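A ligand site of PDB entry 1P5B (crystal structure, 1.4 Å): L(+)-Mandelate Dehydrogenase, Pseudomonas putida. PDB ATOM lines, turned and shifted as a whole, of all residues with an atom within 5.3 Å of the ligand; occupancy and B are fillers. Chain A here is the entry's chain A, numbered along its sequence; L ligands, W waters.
OG of Ser 108 lies within hydrogen-bond range of O2 of the ligand (2.6 Å). OG1 of Thr 156 is in hydrogen-bond range of O1 of the ligand. O of Pro 79 is in hydrogen-bond range of O3 of the ligand, at 2.7 Å. An oxygen (O4) of the ligand lies within hydrogen-bond range of the side-chain carboxylate (OD2) of Asp 284, at 2.8 Å. An oxygen (O7) of the ligand is in hydrogen-bond range of the backbone NH of Gly 286 (2.8 Å). NH1 of Arg 288 is in salt-bridge range of O7 of the ligand, 2.9 Å away. The backbone NH of Gly 81 lies within hydrogen-bond range of a nitrogen (N3) of the ligand. A nitrogen (N2) of the ligand sits close to the side-chain amide nitrogen (NE2) of Gln 129 (2.9 Å). O1 of the ligand sits at hydrogen-bond distance from NZ of Lys 231 (2.9 Å). O8 of the ligand sits at hydrogen-bond distance from N of Arg 308 (3.0 Å). The guanidinium group (NH1) of Arg 308 is in salt-bridge range of an oxygen (O8) of the ligand. OH of Tyr 131 is in hydrogen-bond range of N2 of the ligand, 3.1 Å away. An oxygen (O9) of the ligand sits at hydrogen-bond distance from the backbone NH (N) of Gly 307 (3.2 Å). OG of Ser 253 sits at hydrogen-bond distance from O4 of the ligand (3.3 Å).
The side-chain hydroxyl of Ser 108 is in hydrogen-bond range of the backbone NH of Ala 110. The side-chain amide oxygen (OE1) of Gln 129 sits close to the side-chain hydroxyl (OG1) of Thr 156, 3.2 Å away. The side-chain hydroxyl (OG) of Ser 285 is in hydrogen-bond range of the side-chain carboxylate (OD1) of Asp 284 (2.7 Å). The side-chain carboxylate (OD1) of Asp 284 lies within hydrogen-bond range of the side-chain hydroxyl (OG) of Ser 253, 2.5 Å away. The side-chain hydroxyl of Thr 109 sits at hydrogen-bond distance from the backbone carbonyl oxygen of Gln 129 (2.7 Å). NE of Arg 308 is in hydrogen-bond range of O of Leu 27, at 2.9 Å. N of Tyr 131 is in hydrogen-bond range of OG1 of Thr 109 (3.0 Å). The backbone NH (N) of His 255 lies within hydrogen-bond range of the side-chain hydroxyl (OG) of Ser 253, at 2.9 Å.
NE2 of His 255 sits close to N4 of the ligand. Merely in contact with the ligand: Tyr 26 (3.6 Å), Leu 27 (3.8 Å), Thr 80 (3.4 Å), Gly 256 (3.2 Å), Arg 258 (3.5 Å) and Ser 285 (3.2 Å). The nearest printed residue that does not touch the ligand is Leu 311 (4.1 Å).
Water W5 lies within hydrogen-bond range of an oxygen (O9) of the ligand (2.6 Å), the backbone NH of Ser 285 (2.8 Å) and the backbone carbonyl oxygen of Leu 305 (2.9 Å). Water W4 lies within hydrogen-bond range of an oxygen (O7) of the ligand, the backbone carbonyl oxygen (O) of Gly 256, the backbone NH (N) of Gly 286 and the guanidinium group (NH1) of Arg 308. Water W1 lies within hydrogen-bond range of OD2 of Asp 284 and O3 of the ligand.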
ATOM      1  N   TYR A  26     -15.366  -5.917 -19.492  1.00  0.00           N
ATOM      2  CA  TYR A  26     -14.274  -4.958 -19.665  1.00  0.00           C
ATOM      3  C   TYR A  26     -13.866  -4.445 -18.281  1.00  0.00           C
ATOM      4  O   TYR A  26     -12.681  -4.314 -17.976  1.00  0.00           O
ATOM      5  CB  TYR A  26     -14.740  -3.777 -20.531  1.00  0.00           C
ATOM      6  CG  TYR A  26     -13.929  -2.510 -20.318  1.00  0.00           C
ATOM      7  CD1 TYR A  26     -12.616  -2.413 -20.785  1.00  0.00           C
ATOM      8  CD2 TYR A  26     -14.465  -1.420 -19.626  1.00  0.00           C
ATOM      9  CE1 TYR A  26     -11.852  -1.271 -20.558  1.00  0.00           C
ATOM     10  CE2 TYR A  26     -13.705  -0.269 -19.395  1.00  0.00           C
ATOM     11  CZ  TYR A  26     -12.407  -0.203 -19.863  1.00  0.00           C
ATOM     12  OH  TYR A  26     -11.653   0.924 -19.612  1.00  0.00           O
ATOM     13  N   LEU A  27     -14.878  -4.179 -17.459  1.00  0.00           N
ATOM     14  CA  LEU A  27     -14.669  -3.668 -16.109  1.00  0.00           C
ATOM     15  C   LEU A  27     -14.089  -4.682 -15.132  1.00  0.00           C
ATOM     16  O   LEU A  27     -13.085  -4.421 -14.472  1.00  0.00           O
ATOM     17  CB  LEU A  27     -16.012  -3.162 -15.548  1.00  0.00           C
ATOM     18  CG  LEU A  27     -16.088  -2.893 -14.045  1.00  0.00           C
ATOM     19  CD1 LEU A  27     -15.178  -1.737 -13.682  1.00  0.00           C
ATOM     20  CD2 LEU A  27     -17.520  -2.571 -13.659  1.00  0.00           C
ATOM     21  N   GLY A  78      -9.060   6.384  -7.972  1.00  0.00           N
ATOM     22  CA  GLY A  78      -7.962   6.251  -8.913  1.00  0.00           C
ATOM     23  C   GLY A  78      -8.340   6.436 -10.368  1.00  0.00           C
ATOM     24  O   GLY A  78      -9.511   6.454 -10.721  1.00  0.00           O
ATOM     25  N   PRO A  79      -7.327   6.545 -11.245  1.00  0.00           N
ATOM     26  CA  PRO A  79      -7.556   6.726 -12.675  1.00  0.00           C
ATOM     27  C   PRO A  79      -8.041   5.467 -13.390  1.00  0.00           C
ATOM     28  O   PRO A  79      -7.394   4.432 -13.322  1.00  0.00           O
ATOM     29  CB  PRO A  79      -6.198   7.190 -13.188  1.00  0.00           C
ATOM     30  CG  PRO A  79      -5.252   6.425 -12.304  1.00  0.00           C
ATOM     31  CD  PRO A  79      -5.882   6.564 -10.933  1.00  0.00           C
ATOM     32  N   THR A  80      -9.181   5.579 -14.055  1.00  0.00           N
ATOM     33  CA  THR A  80      -9.718   4.464 -14.819  1.00  0.00           C
ATOM     34  C   THR A  80     -10.233   5.026 -16.140  1.00  0.00           C
ATOM     35  O   THR A  80     -10.932   6.040 -16.165  1.00  0.00           O
ATOM     36  CB  THR A  80     -10.865   3.739 -14.065  1.00  0.00           C
ATOM     37  OG1 THR A  80     -11.892   4.672 -13.712  1.00  0.00           O
ATOM     38  CG2 THR A  80     -10.322   3.074 -12.801  1.00  0.00           C
ATOM     39  N   GLY A  81      -9.874   4.365 -17.238  1.00  0.00           N
ATOM     40  CA  GLY A  81     -10.289   4.843 -18.541  1.00  0.00           C
ATOM     41  C   GLY A  81     -11.660   4.369 -18.985  1.00  0.00           C
ATOM     42  O   GLY A  81     -12.173   3.363 -18.513  1.00  0.00           O
ATOM     43  N   SER A 108      -8.071   9.914 -15.937  1.00  0.00           N
ATOM     44  CA  SER A 108      -7.271   9.056 -16.807  1.00  0.00           C
ATOM     45  C   SER A 108      -6.961   9.745 -18.128  1.00  0.00           C
ATOM     46  O   SER A 108      -7.734  10.574 -18.609  1.00  0.00           O
ATOM     47  CB  SER A 108      -8.032   7.759 -17.108  1.00  0.00           C
ATOM     48  OG  SER A 108      -7.443   7.052 -18.191  1.00  0.00           O
ATOM     49  N   THR A 109      -5.825   9.391 -18.726  1.00  0.00           N
ATOM     50  CA  THR A 109      -5.465   9.943 -20.019  1.00  0.00           C
ATOM     51  C   THR A 109      -6.510   9.459 -21.025  1.00  0.00           C
ATOM     52  O   THR A 109      -6.784  10.119 -22.024  1.00  0.00           O
ATOM     53  CB  THR A 109      -4.068   9.454 -20.464  1.00  0.00           C
ATOM     54  OG1 THR A 109      -3.062  10.191 -19.767  1.00  0.00           O
ATOM     55  CG2 THR A 109      -3.879   9.644 -21.964  1.00  0.00           C
ATOM     56  N   ALA A 110      -7.105   8.298 -20.733  1.00  0.00           N
ATOM     57  CA  ALA A 110      -8.114   7.688 -21.596  1.00  0.00           C
ATOM     58  C   ALA A 110      -9.535   7.989 -21.108  1.00  0.00           C
ATOM     59  O   ALA A 110     -10.445   7.171 -21.276  1.00  0.00           O
ATOM     60  CB  ALA A 110      -7.889   6.185 -21.683  1.00  0.00           C
ATOM     61  N   GLN A 129      -3.639  11.568 -14.504  1.00  0.00           N
ATOM     62  CA  GLN A 129      -2.842  10.374 -14.760  1.00  0.00           C
ATOM     63  C   GLN A 129      -2.409  10.389 -16.214  1.00  0.00           C
ATOM     64  O   GLN A 129      -3.235  10.452 -17.123  1.00  0.00           O
ATOM     65  CB  GLN A 129      -3.656   9.110 -14.463  1.00  0.00           C
ATOM     66  CG  GLN A 129      -2.955   7.813 -14.869  1.00  0.00           C
ATOM     67  CD  GLN A 129      -3.212   7.406 -16.305  1.00  0.00           C
ATOM     68  OE1 GLN A 129      -2.280   7.081 -17.057  1.00  0.00           O
ATOM     69  NE2 GLN A 129      -4.474   7.399 -16.693  1.00  0.00           N
ATOM     70  N   TYR A 131      -0.358   8.839 -19.601  1.00  0.00           N
ATOM     71  CA  TYR A 131       0.088   7.692 -20.385  1.00  0.00           C
ATOM     72  C   TYR A 131       0.846   8.383 -21.510  1.00  0.00           C
ATOM     73  O   TYR A 131       0.357   9.361 -22.080  1.00  0.00           O
ATOM     74  CB  TYR A 131      -1.082   6.933 -21.018  1.00  0.00           C
ATOM     75  CG  TYR A 131      -1.697   5.853 -20.170  1.00  0.00           C
ATOM     76  CD1 TYR A 131      -0.898   4.979 -19.423  1.00  0.00           C
ATOM     77  CD2 TYR A 131      -3.076   5.651 -20.167  1.00  0.00           C
ATOM     78  CE1 TYR A 131      -1.475   3.922 -18.708  1.00  0.00           C
ATOM     79  CE2 TYR A 131      -3.651   4.599 -19.461  1.00  0.00           C
ATOM     80  CZ  TYR A 131      -2.847   3.749 -18.733  1.00  0.00           C
ATOM     81  OH  TYR A 131      -3.412   2.699 -18.047  1.00  0.00           O
ATOM     82  N   THR A 156       1.611   6.558 -15.175  1.00  0.00           N
ATOM     83  CA  THR A 156       1.346   5.117 -15.084  1.00  0.00           C
ATOM     84  C   THR A 156       2.335   4.411 -15.988  1.00  0.00           C
ATOM     85  O   THR A 156       2.382   4.648 -17.198  1.00  0.00           O
ATOM     86  CB  THR A 156      -0.090   4.798 -15.488  1.00  0.00           C
ATOM     87  OG1 THR A 156      -0.986   5.452 -14.586  1.00  0.00           O
ATOM     88  CG2 THR A 156      -0.327   3.299 -15.425  1.00  0.00           C
ATOM     89  N   LYS A 231       3.143   5.478 -10.834  1.00  0.00           N
ATOM     90  CA  LYS A 231       2.194   4.399 -10.576  1.00  0.00           C
ATOM     91  C   LYS A 231       2.519   3.126 -11.337  1.00  0.00           C
ATOM     92  O   LYS A 231       3.022   3.156 -12.457  1.00  0.00           O
ATOM     93  CB  LYS A 231       0.792   4.884 -10.969  1.00  0.00           C
ATOM     94  CG  LYS A 231      -0.342   3.870 -10.871  1.00  0.00           C
ATOM     95  CD  LYS A 231      -1.676   4.594 -11.047  1.00  0.00           C
ATOM     96  CE  LYS A 231      -2.884   3.670 -10.954  1.00  0.00           C
ATOM     97  NZ  LYS A 231      -3.110   2.880 -12.192  1.00  0.00           N
ATOM     98  N   SER A 253       1.191  -0.853  -7.424  1.00  0.00           N
ATOM     99  CA  SER A 253      -0.010  -1.331  -8.096  1.00  0.00           C
ATOM    100  C   SER A 253       0.275  -2.356  -9.182  1.00  0.00           C
ATOM    101  O   SER A 253       1.350  -2.330  -9.780  1.00  0.00           O
ATOM    102  CB  SER A 253      -0.691  -0.110  -8.752  1.00  0.00           C
ATOM    103  OG  SER A 253      -1.706  -0.469  -9.666  1.00  0.00           O
ATOM    104  N   HIS A 255      -2.192  -2.753 -11.442  1.00  0.00           N
ATOM    105  CA  HIS A 255      -3.243  -2.336 -12.352  1.00  0.00           C
ATOM    106  C   HIS A 255      -4.501  -3.185 -12.191  1.00  0.00           C
ATOM    107  O   HIS A 255      -5.176  -3.502 -13.169  1.00  0.00           O
ATOM    108  CB  HIS A 255      -2.726  -2.436 -13.787  1.00  0.00           C
ATOM    109  CG  HIS A 255      -3.280  -1.416 -14.727  1.00  0.00           C
ATOM    110  ND1 HIS A 255      -2.569  -0.298 -15.118  1.00  0.00           N
ATOM    111  CD2 HIS A 255      -4.474  -1.348 -15.378  1.00  0.00           C
ATOM    112  CE1 HIS A 255      -3.291   0.410 -15.971  1.00  0.00           C
ATOM    113  NE2 HIS A 255      -4.453  -0.202 -16.132  1.00  0.00           N
ATOM    114  N   GLY A 256      -4.808  -3.557 -10.949  1.00  0.00           N
ATOM    115  CA  GLY A 256      -5.993  -4.367 -10.700  1.00  0.00           C
ATOM    116  C   GLY A 256      -6.015  -5.712 -11.393  1.00  0.00           C
ATOM    117  O   GLY A 256      -7.072  -6.191 -11.779  1.00  0.00           O
ATOM    118  N   ARG A 258      -5.097  -6.468 -14.268  1.00  0.00           N
ATOM    119  CA  ARG A 258      -5.473  -6.356 -15.671  1.00  0.00           C
ATOM    120  C   ARG A 258      -4.340  -6.408 -16.672  1.00  0.00           C
ATOM    121  O   ARG A 258      -4.594  -6.453 -17.884  1.00  0.00           O
ATOM    122  CB  ARG A 258      -6.250  -5.052 -15.871  1.00  0.00           C
ATOM    123  CG  ARG A 258      -7.512  -4.950 -15.045  1.00  0.00           C
ATOM    124  CD  ARG A 258      -8.059  -3.541 -15.021  1.00  0.00           C
ATOM    125  NE  ARG A 258      -8.547  -3.065 -16.314  1.00  0.00           N
ATOM    126  CZ  ARG A 258      -9.719  -3.386 -16.837  1.00  0.00           C
ATOM    127  NH1 ARG A 258     -10.547  -4.191 -16.185  1.00  0.00           N
ATOM    128  NH2 ARG A 258     -10.095  -2.871 -18.004  1.00  0.00           N
ATOM    129  N   ASP A 284      -2.893   0.508  -4.579  1.00  0.00           N
ATOM    130  CA  ASP A 284      -4.207   0.097  -5.074  1.00  0.00           C
ATOM    131  C   ASP A 284      -4.092  -1.357  -5.491  1.00  0.00           C
ATOM    132  O   ASP A 284      -3.039  -1.977  -5.298  1.00  0.00           O
ATOM    133  CB  ASP A 284      -4.698   0.993  -6.245  1.00  0.00           C
ATOM    134  CG  ASP A 284      -3.932   0.783  -7.540  1.00  0.00           C
ATOM    135  OD1 ASP A 284      -3.330  -0.293  -7.752  1.00  0.00           O
ATOM    136  OD2 ASP A 284      -3.963   1.698  -8.387  1.00  0.00           O
ATOM    137  N   SER A 285      -5.192  -1.895  -6.017  1.00  0.00           N
ATOM    138  CA  SER A 285      -5.286  -3.279  -6.500  1.00  0.00           C
ATOM    139  C   SER A 285      -5.839  -4.290  -5.512  1.00  0.00           C
ATOM    140  O   SER A 285      -5.118  -4.797  -4.653  1.00  0.00           O
ATOM    141  CB  SER A 285      -3.934  -3.783  -7.033  1.00  0.00           C
ATOM    142  OG  SER A 285      -3.489  -3.006  -8.137  1.00  0.00           O
ATOM    143  N   GLY A 286      -7.132  -4.565  -5.649  1.00  0.00           N
ATOM    144  CA  GLY A 286      -7.792  -5.545  -4.802  1.00  0.00           C
ATOM    145  C   GLY A 286      -8.591  -5.044  -3.617  1.00  0.00           C
ATOM    146  O   GLY A 286      -9.240  -5.838  -2.943  1.00  0.00           O
ATOM    147  N   PHE A 287      -8.580  -3.742  -3.365  1.00  0.00           N
ATOM    148  CA  PHE A 287      -9.291  -3.194  -2.217  1.00  0.00           C
ATOM    149  C   PHE A 287     -10.811  -3.166  -2.376  1.00  0.00           C
ATOM    150  O   PHE A 287     -11.331  -2.565  -3.313  1.00  0.00           O
ATOM    151  CB  PHE A 287      -8.757  -1.796  -1.893  1.00  0.00           C
ATOM    152  CG  PHE A 287      -7.317  -1.796  -1.471  1.00  0.00           C
ATOM    153  CD1 PHE A 287      -6.302  -1.796  -2.418  1.00  0.00           C
ATOM    154  CD2 PHE A 287      -6.986  -1.858  -0.114  1.00  0.00           C
ATOM    155  CE1 PHE A 287      -4.965  -1.860  -2.036  1.00  0.00           C
ATOM    156  CE2 PHE A 287      -5.642  -1.925   0.280  1.00  0.00           C
ATOM    157  CZ  PHE A 287      -4.639  -1.933  -0.688  1.00  0.00           C
ATOM    158  N   ARG A 288     -11.503  -3.814  -1.449  1.00  0.00           N
ATOM    159  CA  ARG A 288     -12.966  -3.888  -1.492  1.00  0.00           C
ATOM    160  C   ARG A 288     -13.637  -3.612  -0.145  1.00  0.00           C
ATOM    161  O   ARG A 288     -14.733  -3.065  -0.104  1.00  0.00           O
ATOM    162  CB  ARG A 288     -13.412  -5.263  -1.982  1.00  0.00           C
ATOM    163  CG  ARG A 288     -12.868  -5.663  -3.341  1.00  0.00           C
ATOM    164  CD  ARG A 288     -13.505  -4.881  -4.489  1.00  0.00           C
ATOM    165  NE  ARG A 288     -13.031  -5.370  -5.782  1.00  0.00           N
ATOM    166  CZ  ARG A 288     -11.878  -5.015  -6.338  1.00  0.00           C
ATOM    167  NH1 ARG A 288     -11.064  -4.160  -5.720  1.00  0.00           N
ATOM    168  NH2 ARG A 288     -11.507  -5.546  -7.496  1.00  0.00           N
ATOM    169  N   LEU A 305      -5.948   3.915  -3.314  1.00  0.00           N
ATOM    170  CA  LEU A 305      -6.739   4.379  -4.448  1.00  0.00           C
ATOM    171  C   LEU A 305      -7.739   3.295  -4.796  1.00  0.00           C
ATOM    172  O   LEU A 305      -7.412   2.107  -4.817  1.00  0.00           O
ATOM    173  CB  LEU A 305      -5.867   4.678  -5.674  1.00  0.00           C
ATOM    174  CG  LEU A 305      -4.887   5.836  -5.572  1.00  0.00           C
ATOM    175  CD1 LEU A 305      -3.566   5.324  -5.027  1.00  0.00           C
ATOM    176  CD2 LEU A 305      -4.680   6.474  -6.937  1.00  0.00           C
ATOM    177  N   LEU A 306      -8.973   3.711  -5.062  1.00  0.00           N
ATOM    178  CA  LEU A 306     -10.022   2.794  -5.430  1.00  0.00           C
ATOM    179  C   LEU A 306     -10.168   2.746  -6.930  1.00  0.00           C
ATOM    180  O   LEU A 306     -10.113   3.776  -7.610  1.00  0.00           O
ATOM    181  CB  LEU A 306     -11.353   3.234  -4.820  1.00  0.00           C
ATOM    182  CG  LEU A 306     -11.389   3.379  -3.297  1.00  0.00           C
ATOM    183  CD1 LEU A 306     -12.732   3.926  -2.870  1.00  0.00           C
ATOM    184  CD2 LEU A 306     -11.121   2.032  -2.646  1.00  0.00           C
ATOM    185  N   GLY A 307     -10.330   1.539  -7.446  1.00  0.00           N
ATOM    186  CA  GLY A 307     -10.516   1.336  -8.862  1.00  0.00           C
ATOM    187  C   GLY A 307     -11.925   0.830  -9.079  1.00  0.00           C
ATOM    188  O   GLY A 307     -12.874   1.597  -9.154  1.00  0.00           O
ATOM    189  N   ARG A 308     -12.068  -0.488  -9.126  1.00  0.00           N
ATOM    190  CA  ARG A 308     -13.384  -1.079  -9.353  1.00  0.00           C
ATOM    191  C   ARG A 308     -14.433  -0.780  -8.286  1.00  0.00           C
ATOM    192  O   ARG A 308     -15.606  -0.671  -8.605  1.00  0.00           O
ATOM    193  CB  ARG A 308     -13.263  -2.586  -9.529  1.00  0.00           C
ATOM    194  CG  ARG A 308     -12.525  -3.022 -10.781  1.00  0.00           C
ATOM    195  CD  ARG A 308     -12.603  -4.531 -10.942  1.00  0.00           C
ATOM    196  NE  ARG A 308     -11.788  -5.088 -12.021  1.00  0.00           N
ATOM    197  CZ  ARG A 308     -10.486  -5.347 -11.941  1.00  0.00           C
ATOM    198  NH1 ARG A 308      -9.823  -5.093 -10.821  1.00  0.00           N
ATOM    199  NH2 ARG A 308      -9.876  -5.930 -12.961  1.00  0.00           N
ATOM    200  N   ALA A 309     -14.025  -0.665  -7.024  1.00  0.00           N
ATOM    201  CA  ALA A 309     -15.005  -0.433  -5.952  1.00  0.00           C
ATOM    202  C   ALA A 309     -15.966   0.708  -6.261  1.00  0.00           C
ATOM    203  O   ALA A 309     -17.179   0.537  -6.216  1.00  0.00           O
ATOM    204  CB  ALA A 309     -14.292  -0.196  -4.626  1.00  0.00           C
ATOM    205  N   LEU A 311     -16.260   2.158  -9.178  1.00  0.00           N
ATOM    206  CA  LEU A 311     -16.835   1.974 -10.507  1.00  0.00           C
ATOM    207  C   LEU A 311     -18.108   1.141 -10.416  1.00  0.00           C
ATOM    208  O   LEU A 311     -18.999   1.281 -11.250  1.00  0.00           O
ATOM    209  CB  LEU A 311     -15.831   1.326 -11.468  1.00  0.00           C
ATOM    210  CG  LEU A 311     -14.653   2.208 -11.872  1.00  0.00           C
ATOM    211  CD1 LEU A 311     -13.822   1.495 -12.935  1.00  0.00           C
ATOM    212  CD2 LEU A 311     -15.157   3.550 -12.411  1.00  0.00           C
HETATM  213  N1  LIG L   1      -4.959   2.871 -14.517  1.00  0.00           N
HETATM  214  C1  LIG L   1      -4.398   4.016 -15.031  1.00  0.00           C
HETATM  215  O1  LIG L   1      -3.471   4.508 -14.571  1.00  0.00           O
HETATM  216  N2  LIG L   1      -5.086   4.604 -16.198  1.00  0.00           N
HETATM  217  C2  LIG L   1      -6.231   4.079 -16.869  1.00  0.00           C
HETATM  218  O2  LIG L   1      -6.758   4.619 -17.811  1.00  0.00           O
HETATM  219  C3  LIG L   1      -6.820   2.850 -16.283  1.00  0.00           C
HETATM  220  N3  LIG L   1      -7.972   2.291 -16.741  1.00  0.00           N
HETATM  221  C4  LIG L   1      -8.647   1.290 -16.038  1.00  0.00           C
HETATM  222  C5  LIG L   1      -9.949   0.858 -16.479  1.00  0.00           C
HETATM  223  C6  LIG L   1     -10.758  -0.104 -15.661  1.00  0.00           C
HETATM  224  C7  LIG L   1     -12.114  -0.456 -16.120  1.00  0.00           C
HETATM  225  C8  LIG L   1     -10.142  -0.671 -14.357  1.00  0.00           C
HETATM  226  C9  LIG L   1     -10.816  -1.594 -13.416  1.00  0.00           C
HETATM  227  C10 LIG L   1      -8.861  -0.266 -13.977  1.00  0.00           C
HETATM  228  C11 LIG L   1      -8.040   0.707 -14.734  1.00  0.00           C
HETATM  229  N4  LIG L   1      -6.737   1.263 -14.349  1.00  0.00           N
HETATM  230  C12 LIG L   1      -6.074   2.334 -15.036  1.00  0.00           C
HETATM  231  C13 LIG L   1      -6.116   0.733 -13.118  1.00  0.00           C
HETATM  232  C14 LIG L   1      -6.585   1.453 -11.847  1.00  0.00           C
HETATM  233  O3  LIG L   1      -6.017   2.704 -11.756  1.00  0.00           O
HETATM  234  C15 LIG L   1      -6.224   0.678 -10.581  1.00  0.00           C
HETATM  235  O4  LIG L   1      -4.792   0.324 -10.628  1.00  0.00           O
HETATM  236  C16 LIG L   1      -6.933  -0.682 -10.408  1.00  0.00           C
HETATM  237  O5  LIG L   1      -8.306  -0.562 -10.765  1.00  0.00           O
HETATM  238  C17 LIG L   1      -6.810  -1.055  -8.953  1.00  0.00           C
HETATM  239  O6  LIG L   1      -7.463  -2.330  -8.656  1.00  0.00           O
HETATM  240  P1  LIG L   1      -8.954  -2.562  -8.251  1.00  0.00           P
HETATM  241  O7  LIG L   1      -8.982  -3.965  -7.667  1.00  0.00           O
HETATM  242  O8  LIG L   1      -9.790  -2.428  -9.516  1.00  0.00           O
HETATM  243  O9  LIG L   1      -9.297  -1.512  -7.220  1.00  0.00           O
HETATM  244  O   HOH W   1      -5.882   3.732  -9.015  1.00  0.00           O
HETATM  245  O   HOH W   2     -13.856   2.395 -16.479  1.00  0.00           O
HETATM  246  O   HOH W   3     -11.367  -0.751  -5.718  1.00  0.00           O
HETATM  247  O   HOH W   4      -7.626  -6.276  -8.512  1.00  0.00           O
HETATM  248  O   HOH W   5      -7.661  -0.739  -5.308  1.00  0.00           O
HETATM  249  O   HOH W   6      -7.425   3.089 -19.921  1.00  0.00           O
